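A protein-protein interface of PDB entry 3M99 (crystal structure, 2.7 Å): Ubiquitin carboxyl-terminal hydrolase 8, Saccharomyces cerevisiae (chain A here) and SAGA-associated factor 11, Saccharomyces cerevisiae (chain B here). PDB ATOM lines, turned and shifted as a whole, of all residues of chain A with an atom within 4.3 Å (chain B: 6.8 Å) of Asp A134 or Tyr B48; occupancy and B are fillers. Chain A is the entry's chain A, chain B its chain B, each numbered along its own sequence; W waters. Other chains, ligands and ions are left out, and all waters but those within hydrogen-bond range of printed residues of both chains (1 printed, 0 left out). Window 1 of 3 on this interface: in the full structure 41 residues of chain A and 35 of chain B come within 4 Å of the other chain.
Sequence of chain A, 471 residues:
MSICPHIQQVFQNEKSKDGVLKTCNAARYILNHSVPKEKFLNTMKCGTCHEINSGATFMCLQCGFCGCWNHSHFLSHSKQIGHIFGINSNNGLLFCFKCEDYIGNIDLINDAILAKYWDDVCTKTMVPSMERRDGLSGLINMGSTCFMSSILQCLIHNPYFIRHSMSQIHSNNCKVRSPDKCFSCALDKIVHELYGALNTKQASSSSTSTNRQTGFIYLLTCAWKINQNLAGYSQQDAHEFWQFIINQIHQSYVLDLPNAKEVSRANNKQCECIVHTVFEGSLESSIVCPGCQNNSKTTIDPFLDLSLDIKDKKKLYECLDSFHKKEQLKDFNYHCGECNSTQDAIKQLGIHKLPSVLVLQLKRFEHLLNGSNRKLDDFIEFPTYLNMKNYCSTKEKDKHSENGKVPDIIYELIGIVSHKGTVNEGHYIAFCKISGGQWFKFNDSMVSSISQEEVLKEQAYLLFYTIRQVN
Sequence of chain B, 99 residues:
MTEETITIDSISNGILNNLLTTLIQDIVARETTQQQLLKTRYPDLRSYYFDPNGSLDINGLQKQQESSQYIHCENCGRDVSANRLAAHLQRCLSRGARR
The side-chain carboxylate (OD2) of Asp A134 lies within hydrogen-bond range of the side-chain hydroxyl (OH) of Tyr B48 (3.0 Å).
The guanidinium group (NH2) of Arg A132 lies within hydrogen-bond range of the backbone carbonyl oxygen (O) of Leu A136 (2.9 Å). The guanidinium group (NE) of Arg A133 lies within salt-bridge range of the side-chain carboxylate (OD2) of Asp A134, at 3.9 Å.
Among the printed residues, merely in contact across the chains: Arg A133 with Tyr B48 (3.6 Å), Leu A136 with Tyr B48 (3.5 Å), Leu A136 with Ile B58 (3.95 Å), Phe A440 with Tyr B48 (3.8 Å) and Phe A440 with Ile B58 (3.9 Å).
Asp A134 touches just one residue of chain B: Tyr B48. Tyr B48 touches four residues of chain A. Of the printed residues of chain A, Ile B58 touches Leu A136 and Phe A440. Printed residues of chain B within 4 Å of Phe A440: Tyr B48 (3.8 Å) and Ile B58 (3.9 Å). Of the printed residues of chain B, Arg A133 touches Tyr B48. Of the printed residues of chain B, Leu A136 touches Tyr B48 and Ile B58. Gly A135 touches none of the printed residues of chain B. Tyr B49 touches none of the printed residues of chain A. The nearest printed residue of chain B that does not touch Leu A136 is Asn B59 (7.0 Å).
Of the 9 printed residues of chain A, 4 touch a printed residue of chain B. Hydrophobic or aromatic side chains of chain A within 4 Å of the printed part of chain B: Leu A136 and Phe A440. Among the printed residues, no Asp or Glu carboxylate lies within 4 Å of a Lys or Arg side-chain nitrogen of the other chain.
Water W1 bridges the side-chain hydroxyl of Tyr B48 and the backbone NH of Asp A134.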
ATOM      1  N   ARG A 132     -11.854  16.831  -1.357  1.00  0.00           N
ATOM      2  CA  ARG A 132     -12.290  16.196  -0.123  1.00  0.00           C
ATOM      3  C   ARG A 132     -12.431  14.685  -0.207  1.00  0.00           C
ATOM      4  O   ARG A 132     -12.849  14.059   0.761  1.00  0.00           O
ATOM      5  CB  ARG A 132     -13.622  16.798   0.333  1.00  0.00           C
ATOM      6  CG  ARG A 132     -13.513  18.226   0.849  1.00  0.00           C
ATOM      7  CD  ARG A 132     -12.747  18.307   2.168  1.00  0.00           C
ATOM      8  NE  ARG A 132     -11.310  18.075   2.016  1.00  0.00           N
ATOM      9  CZ  ARG A 132     -10.453  18.971   1.536  1.00  0.00           C
ATOM     10  NH1 ARG A 132     -10.883  20.165   1.145  1.00  0.00           N
ATOM     11  NH2 ARG A 132      -9.165  18.670   1.436  1.00  0.00           N
ATOM     12  N   ARG A 133     -12.075  14.097  -1.346  1.00  0.00           N
ATOM     13  CA  ARG A 133     -12.410  12.692  -1.627  1.00  0.00           C
ATOM     14  C   ARG A 133     -11.605  11.677  -0.817  1.00  0.00           C
ATOM     15  O   ARG A 133     -12.006  10.520  -0.689  1.00  0.00           O
ATOM     16  CB  ARG A 133     -12.253  12.387  -3.118  1.00  0.00           C
ATOM     17  CG  ARG A 133     -10.826  12.056  -3.552  1.00  0.00           C
ATOM     18  CD  ARG A 133     -10.745  11.897  -5.061  1.00  0.00           C
ATOM     19  NE  ARG A 133      -9.412  11.542  -5.538  1.00  0.00           N
ATOM     20  CZ  ARG A 133      -8.431  12.415  -5.736  1.00  0.00           C
ATOM     21  NH1 ARG A 133      -8.620  13.704  -5.479  1.00  0.00           N
ATOM     22  NH2 ARG A 133      -7.255  11.994  -6.180  1.00  0.00           N
ATOM     23  N   ASP A 134     -10.462  12.104  -0.289  1.00  0.00           N
ATOM     24  CA  ASP A 134      -9.589  11.200   0.446  1.00  0.00           C
ATOM     25  C   ASP A 134      -9.501  11.641   1.905  1.00  0.00           C
ATOM     26  O   ASP A 134      -8.724  11.101   2.699  1.00  0.00           O
ATOM     27  CB  ASP A 134      -8.206  11.136  -0.211  1.00  0.00           C
ATOM     28  CG  ASP A 134      -8.232  10.425  -1.568  1.00  0.00           C
ATOM     29  OD1 ASP A 134      -9.165   9.624  -1.793  1.00  0.00           O
ATOM     30  OD2 ASP A 134      -7.326  10.653  -2.408  1.00  0.00           O
ATOM     31  N   GLY A 135     -10.327  12.622   2.250  1.00  0.00           N
ATOM     32  CA  GLY A 135     -10.349  13.158   3.594  1.00  0.00           C
ATOM     33  C   GLY A 135      -8.971  13.613   4.018  1.00  0.00           C
ATOM     34  O   GLY A 135      -8.609  13.506   5.189  1.00  0.00           O
ATOM     35  N   LEU A 136      -8.193  14.109   3.063  1.00  0.00           N
ATOM     36  CA  LEU A 136      -6.867  14.618   3.363  1.00  0.00           C
ATOM     37  C   LEU A 136      -6.971  16.077   3.769  1.00  0.00           C
ATOM     38  O   LEU A 136      -7.396  16.918   2.977  1.00  0.00           O
ATOM     39  CB  LEU A 136      -5.945  14.463   2.160  1.00  0.00           C
ATOM     40  CG  LEU A 136      -5.470  13.035   1.901  1.00  0.00           C
ATOM     41  CD1 LEU A 136      -4.867  12.899   0.511  1.00  0.00           C
ATOM     42  CD2 LEU A 136      -4.474  12.608   2.959  1.00  0.00           C
ATOM     43  N   HIS A 157      -8.539   8.016   9.204  1.00  0.00           N
ATOM     44  CA  HIS A 157      -8.152   7.357   7.950  1.00  0.00           C
ATOM     45  C   HIS A 157      -8.131   5.838   8.078  1.00  0.00           C
ATOM     46  O   HIS A 157      -7.490   5.139   7.291  1.00  0.00           O
ATOM     47  CB  HIS A 157      -6.797   7.864   7.459  1.00  0.00           C
ATOM     48  CG  HIS A 157      -6.848   9.239   6.870  1.00  0.00           C
ATOM     49  ND1 HIS A 157      -7.137   9.466   5.541  1.00  0.00           N
ATOM     50  CD2 HIS A 157      -6.652  10.455   7.428  1.00  0.00           C
ATOM     51  CE1 HIS A 157      -7.116  10.766   5.306  1.00  0.00           C
ATOM     52  NE2 HIS A 157      -6.825  11.390   6.434  1.00  0.00           N
ATOM     53  N   TYR A 195     -14.688  14.875   4.672  1.00  0.00           N
ATOM     54  CA  TYR A 195     -15.095  14.098   3.511  1.00  0.00           C
ATOM     55  C   TYR A 195     -16.289  14.757   2.828  1.00  0.00           C
ATOM     56  O   TYR A 195     -16.674  14.357   1.735  1.00  0.00           O
ATOM     57  CB  TYR A 195     -15.477  12.671   3.923  1.00  0.00           C
ATOM     58  CG  TYR A 195     -14.313  11.794   4.321  1.00  0.00           C
ATOM     59  CD1 TYR A 195     -13.833  11.787   5.620  1.00  0.00           C
ATOM     60  CD2 TYR A 195     -13.699  10.967   3.397  1.00  0.00           C
ATOM     61  CE1 TYR A 195     -12.773  10.987   5.982  1.00  0.00           C
ATOM     62  CE2 TYR A 195     -12.639  10.169   3.752  1.00  0.00           C
ATOM     63  CZ  TYR A 195     -12.182  10.184   5.046  1.00  0.00           C
ATOM     64  OH  TYR A 195     -11.127   9.389   5.410  1.00  0.00           O
ATOM     65  N   ILE A 434      -3.193   5.472   2.183  1.00  0.00           N
ATOM     66  CA  ILE A 434      -4.469   5.645   1.508  1.00  0.00           C
ATOM     67  C   ILE A 434      -4.557   4.614   0.382  1.00  0.00           C
ATOM     68  O   ILE A 434      -3.533   4.116  -0.087  1.00  0.00           O
ATOM     69  CB  ILE A 434      -4.591   7.106   0.974  1.00  0.00           C
ATOM     70  CG1 ILE A 434      -5.169   8.030   2.054  1.00  0.00           C
ATOM     71  CG2 ILE A 434      -5.431   7.186  -0.276  1.00  0.00           C
ATOM     72  CD1 ILE A 434      -6.634   7.787   2.366  1.00  0.00           C
ATOM     73  N   PHE A 440       0.929   9.519   3.406  1.00  0.00           N
ATOM     74  CA  PHE A 440       0.885  10.943   3.721  1.00  0.00           C
ATOM     75  C   PHE A 440       1.433  11.247   5.126  1.00  0.00           C
ATOM     76  O   PHE A 440       1.214  10.485   6.068  1.00  0.00           O
ATOM     77  CB  PHE A 440      -0.531  11.496   3.532  1.00  0.00           C
ATOM     78  CG  PHE A 440      -1.054  11.351   2.133  1.00  0.00           C
ATOM     79  CD1 PHE A 440      -1.954  10.350   1.813  1.00  0.00           C
ATOM     80  CD2 PHE A 440      -0.634  12.208   1.129  1.00  0.00           C
ATOM     81  CE1 PHE A 440      -2.433  10.216   0.512  1.00  0.00           C
ATOM     82  CE2 PHE A 440      -1.109  12.078  -0.171  1.00  0.00           C
ATOM     83  CZ  PHE A 440      -2.007  11.083  -0.479  1.00  0.00           C
ATOM     84  N   ARG B  46      -6.525  17.127 -10.144  1.00  0.00           N
ATOM     85  CA  ARG B  46      -5.279  17.604  -9.558  1.00  0.00           C
ATOM     86  C   ARG B  46      -4.683  16.480  -8.716  1.00  0.00           C
ATOM     87  O   ARG B  46      -5.229  16.124  -7.669  1.00  0.00           O
ATOM     88  CB  ARG B  46      -5.502  18.857  -8.692  1.00  0.00           C
ATOM     89  CG  ARG B  46      -6.144  20.039  -9.415  1.00  0.00           C
ATOM     90  CD  ARG B  46      -5.978  21.351  -8.641  1.00  0.00           C
ATOM     91  NE  ARG B  46      -6.782  21.425  -7.416  1.00  0.00           N
ATOM     92  CZ  ARG B  46      -6.694  22.408  -6.520  1.00  0.00           C
ATOM     93  NH1 ARG B  46      -5.837  23.404  -6.705  1.00  0.00           N
ATOM     94  NH2 ARG B  46      -7.460  22.402  -5.433  1.00  0.00           N
ATOM     95  N   SER B  47      -3.580  15.902  -9.183  1.00  0.00           N
ATOM     96  CA  SER B  47      -2.852  14.924  -8.383  1.00  0.00           C
ATOM     97  C   SER B  47      -2.175  15.630  -7.205  1.00  0.00           C
ATOM     98  O   SER B  47      -2.052  16.855  -7.193  1.00  0.00           O
ATOM     99  CB  SER B  47      -1.819  14.180  -9.230  1.00  0.00           C
ATOM    100  OG  SER B  47      -0.714  15.012  -9.524  1.00  0.00           O
ATOM    101  N   TYR B  48      -1.748  14.857  -6.213  1.00  0.00           N
ATOM    102  CA  TYR B  48      -1.136  15.435  -5.020  1.00  0.00           C
ATOM    103  C   TYR B  48       0.331  15.794  -5.253  1.00  0.00           C
ATOM    104  O   TYR B  48       1.115  14.975  -5.731  1.00  0.00           O
ATOM    105  CB  TYR B  48      -1.289  14.493  -3.819  1.00  0.00           C
ATOM    106  CG  TYR B  48      -2.733  14.226  -3.454  1.00  0.00           C
ATOM    107  CD1 TYR B  48      -3.272  12.948  -3.535  1.00  0.00           C
ATOM    108  CD2 TYR B  48      -3.559  15.261  -3.045  1.00  0.00           C
ATOM    109  CE1 TYR B  48      -4.590  12.715  -3.203  1.00  0.00           C
ATOM    110  CE2 TYR B  48      -4.873  15.036  -2.715  1.00  0.00           C
ATOM    111  CZ  TYR B  48      -5.385  13.768  -2.796  1.00  0.00           C
ATOM    112  OH  TYR B  48      -6.704  13.566  -2.465  1.00  0.00           O
ATOM    113  N   TYR B  49       0.681  17.030  -4.911  1.00  0.00           N
ATOM    114  CA  TYR B  49       2.022  17.562  -5.116  1.00  0.00           C
ATOM    115  C   TYR B  49       3.062  16.864  -4.250  1.00  0.00           C
ATOM    116  O   TYR B  49       2.863  16.664  -3.054  1.00  0.00           O
ATOM    117  CB  TYR B  49       2.040  19.069  -4.843  1.00  0.00           C
ATOM    118  CG  TYR B  49       3.339  19.736  -5.221  1.00  0.00           C
ATOM    119  CD1 TYR B  49       3.465  20.442  -6.411  1.00  0.00           C
ATOM    120  CD2 TYR B  49       4.445  19.650  -4.393  1.00  0.00           C
ATOM    121  CE1 TYR B  49       4.662  21.052  -6.760  1.00  0.00           C
ATOM    122  CE2 TYR B  49       5.641  20.253  -4.732  1.00  0.00           C
ATOM    123  CZ  TYR B  49       5.747  20.952  -5.914  1.00  0.00           C
ATOM    124  OH  TYR B  49       6.943  21.548  -6.242  1.00  0.00           O
ATOM    125  N   PHE B  50       4.178  16.501  -4.868  1.00  0.00           N
ATOM    126  CA  PHE B  50       5.263  15.850  -4.154  1.00  0.00           C
ATOM    127  C   PHE B  50       6.545  16.675  -4.182  1.00  0.00           C
ATOM    128  O   PHE B  50       7.444  16.427  -4.982  1.00  0.00           O
ATOM    129  CB  PHE B  50       5.522  14.451  -4.711  1.00  0.00           C
ATOM    130  CG  PHE B  50       6.716  13.771  -4.101  1.00  0.00           C
ATOM    131  CD1 PHE B  50       6.686  13.342  -2.783  1.00  0.00           C
ATOM    132  CD2 PHE B  50       7.868  13.557  -4.844  1.00  0.00           C
ATOM    133  CE1 PHE B  50       7.773  12.717  -2.220  1.00  0.00           C
ATOM    134  CE2 PHE B  50       8.963  12.930  -4.280  1.00  0.00           C
ATOM    135  CZ  PHE B  50       8.913  12.510  -2.964  1.00  0.00           C
ATOM    136  N   ASP B  51       6.612  17.664  -3.299  1.00  0.00           N
ATOM    137  CA  ASP B  51       7.843  18.398  -3.065  1.00  0.00           C
ATOM    138  C   ASP B  51       8.862  17.429  -2.480  1.00  0.00           C
ATOM    139  O   ASP B  51       8.583  16.763  -1.480  1.00  0.00           O
ATOM    140  CB  ASP B  51       7.576  19.552  -2.096  1.00  0.00           C
ATOM    141  CG  ASP B  51       8.837  20.274  -1.675  1.00  0.00           C
ATOM    142  OD1 ASP B  51       8.783  21.005  -0.663  1.00  0.00           O
ATOM    143  OD2 ASP B  51       9.876  20.112  -2.350  1.00  0.00           O
ATOM    144  N   ASP B  57       2.915  21.444   0.780  1.00  0.00           N
ATOM    145  CA  ASP B  57       1.667  20.718   0.946  1.00  0.00           C
ATOM    146  C   ASP B  57       1.451  19.599  -0.054  1.00  0.00           C
ATOM    147  O   ASP B  57       2.240  19.395  -0.979  1.00  0.00           O
ATOM    148  CB  ASP B  57       0.506  21.689   0.763  1.00  0.00           C
ATOM    149  CG  ASP B  57      -0.051  22.182   2.066  1.00  0.00           C
ATOM    150  OD1 ASP B  57       0.364  21.659   3.121  1.00  0.00           O
ATOM    151  OD2 ASP B  57      -0.921  23.081   2.025  1.00  0.00           O
ATOM    152  N   ILE B  58       0.341  18.893   0.138  1.00  0.00           N
ATOM    153  CA  ILE B  58      -0.160  17.963  -0.855  1.00  0.00           C
ATOM    154  C   ILE B  58      -0.561  18.758  -2.079  1.00  0.00           C
ATOM    155  O   ILE B  58      -0.434  18.280  -3.201  1.00  0.00           O
ATOM    156  CB  ILE B  58      -1.364  17.165  -0.343  1.00  0.00           C
ATOM    157  CG1 ILE B  58      -2.340  18.081   0.399  1.00  0.00           C
ATOM    158  CG2 ILE B  58      -0.895  16.040   0.551  1.00  0.00           C
ATOM    159  CD1 ILE B  58      -3.555  17.363   0.930  1.00  0.00           C
ATOM    160  N   ASN B  59      -1.046  19.977  -1.872  1.00  0.00           N
ATOM    161  CA  ASN B  59      -1.273  20.866  -3.007  1.00  0.00           C
ATOM    162  C   ASN B  59      -0.231  21.981  -3.081  1.00  0.00           C
ATOM    163  O   ASN B  59      -0.546  23.130  -3.381  1.00  0.00           O
ATOM    164  CB  ASN B  59      -2.710  21.400  -3.055  1.00  0.00           C
ATOM    165  CG  ASN B  59      -3.201  21.873  -1.716  1.00  0.00           C
ATOM    166  OD1 ASN B  59      -2.473  22.531  -0.979  1.00  0.00           O
ATOM    167  ND2 ASN B  59      -4.446  21.541  -1.387  1.00  0.00           N
ATOM    168  N   GLY B  60       1.014  21.608  -2.793  1.00  0.00           N
ATOM    169  CA  GLY B  60       2.172  22.454  -3.020  1.00  0.00           C
ATOM    170  C   GLY B  60       2.157  23.839  -2.406  1.00  0.00           C
ATOM    171  O   GLY B  60       2.568  24.807  -3.040  1.00  0.00           O
HETATM  172  O   HOH W   1      -8.304  14.462  -0.551  1.00  0.00           O
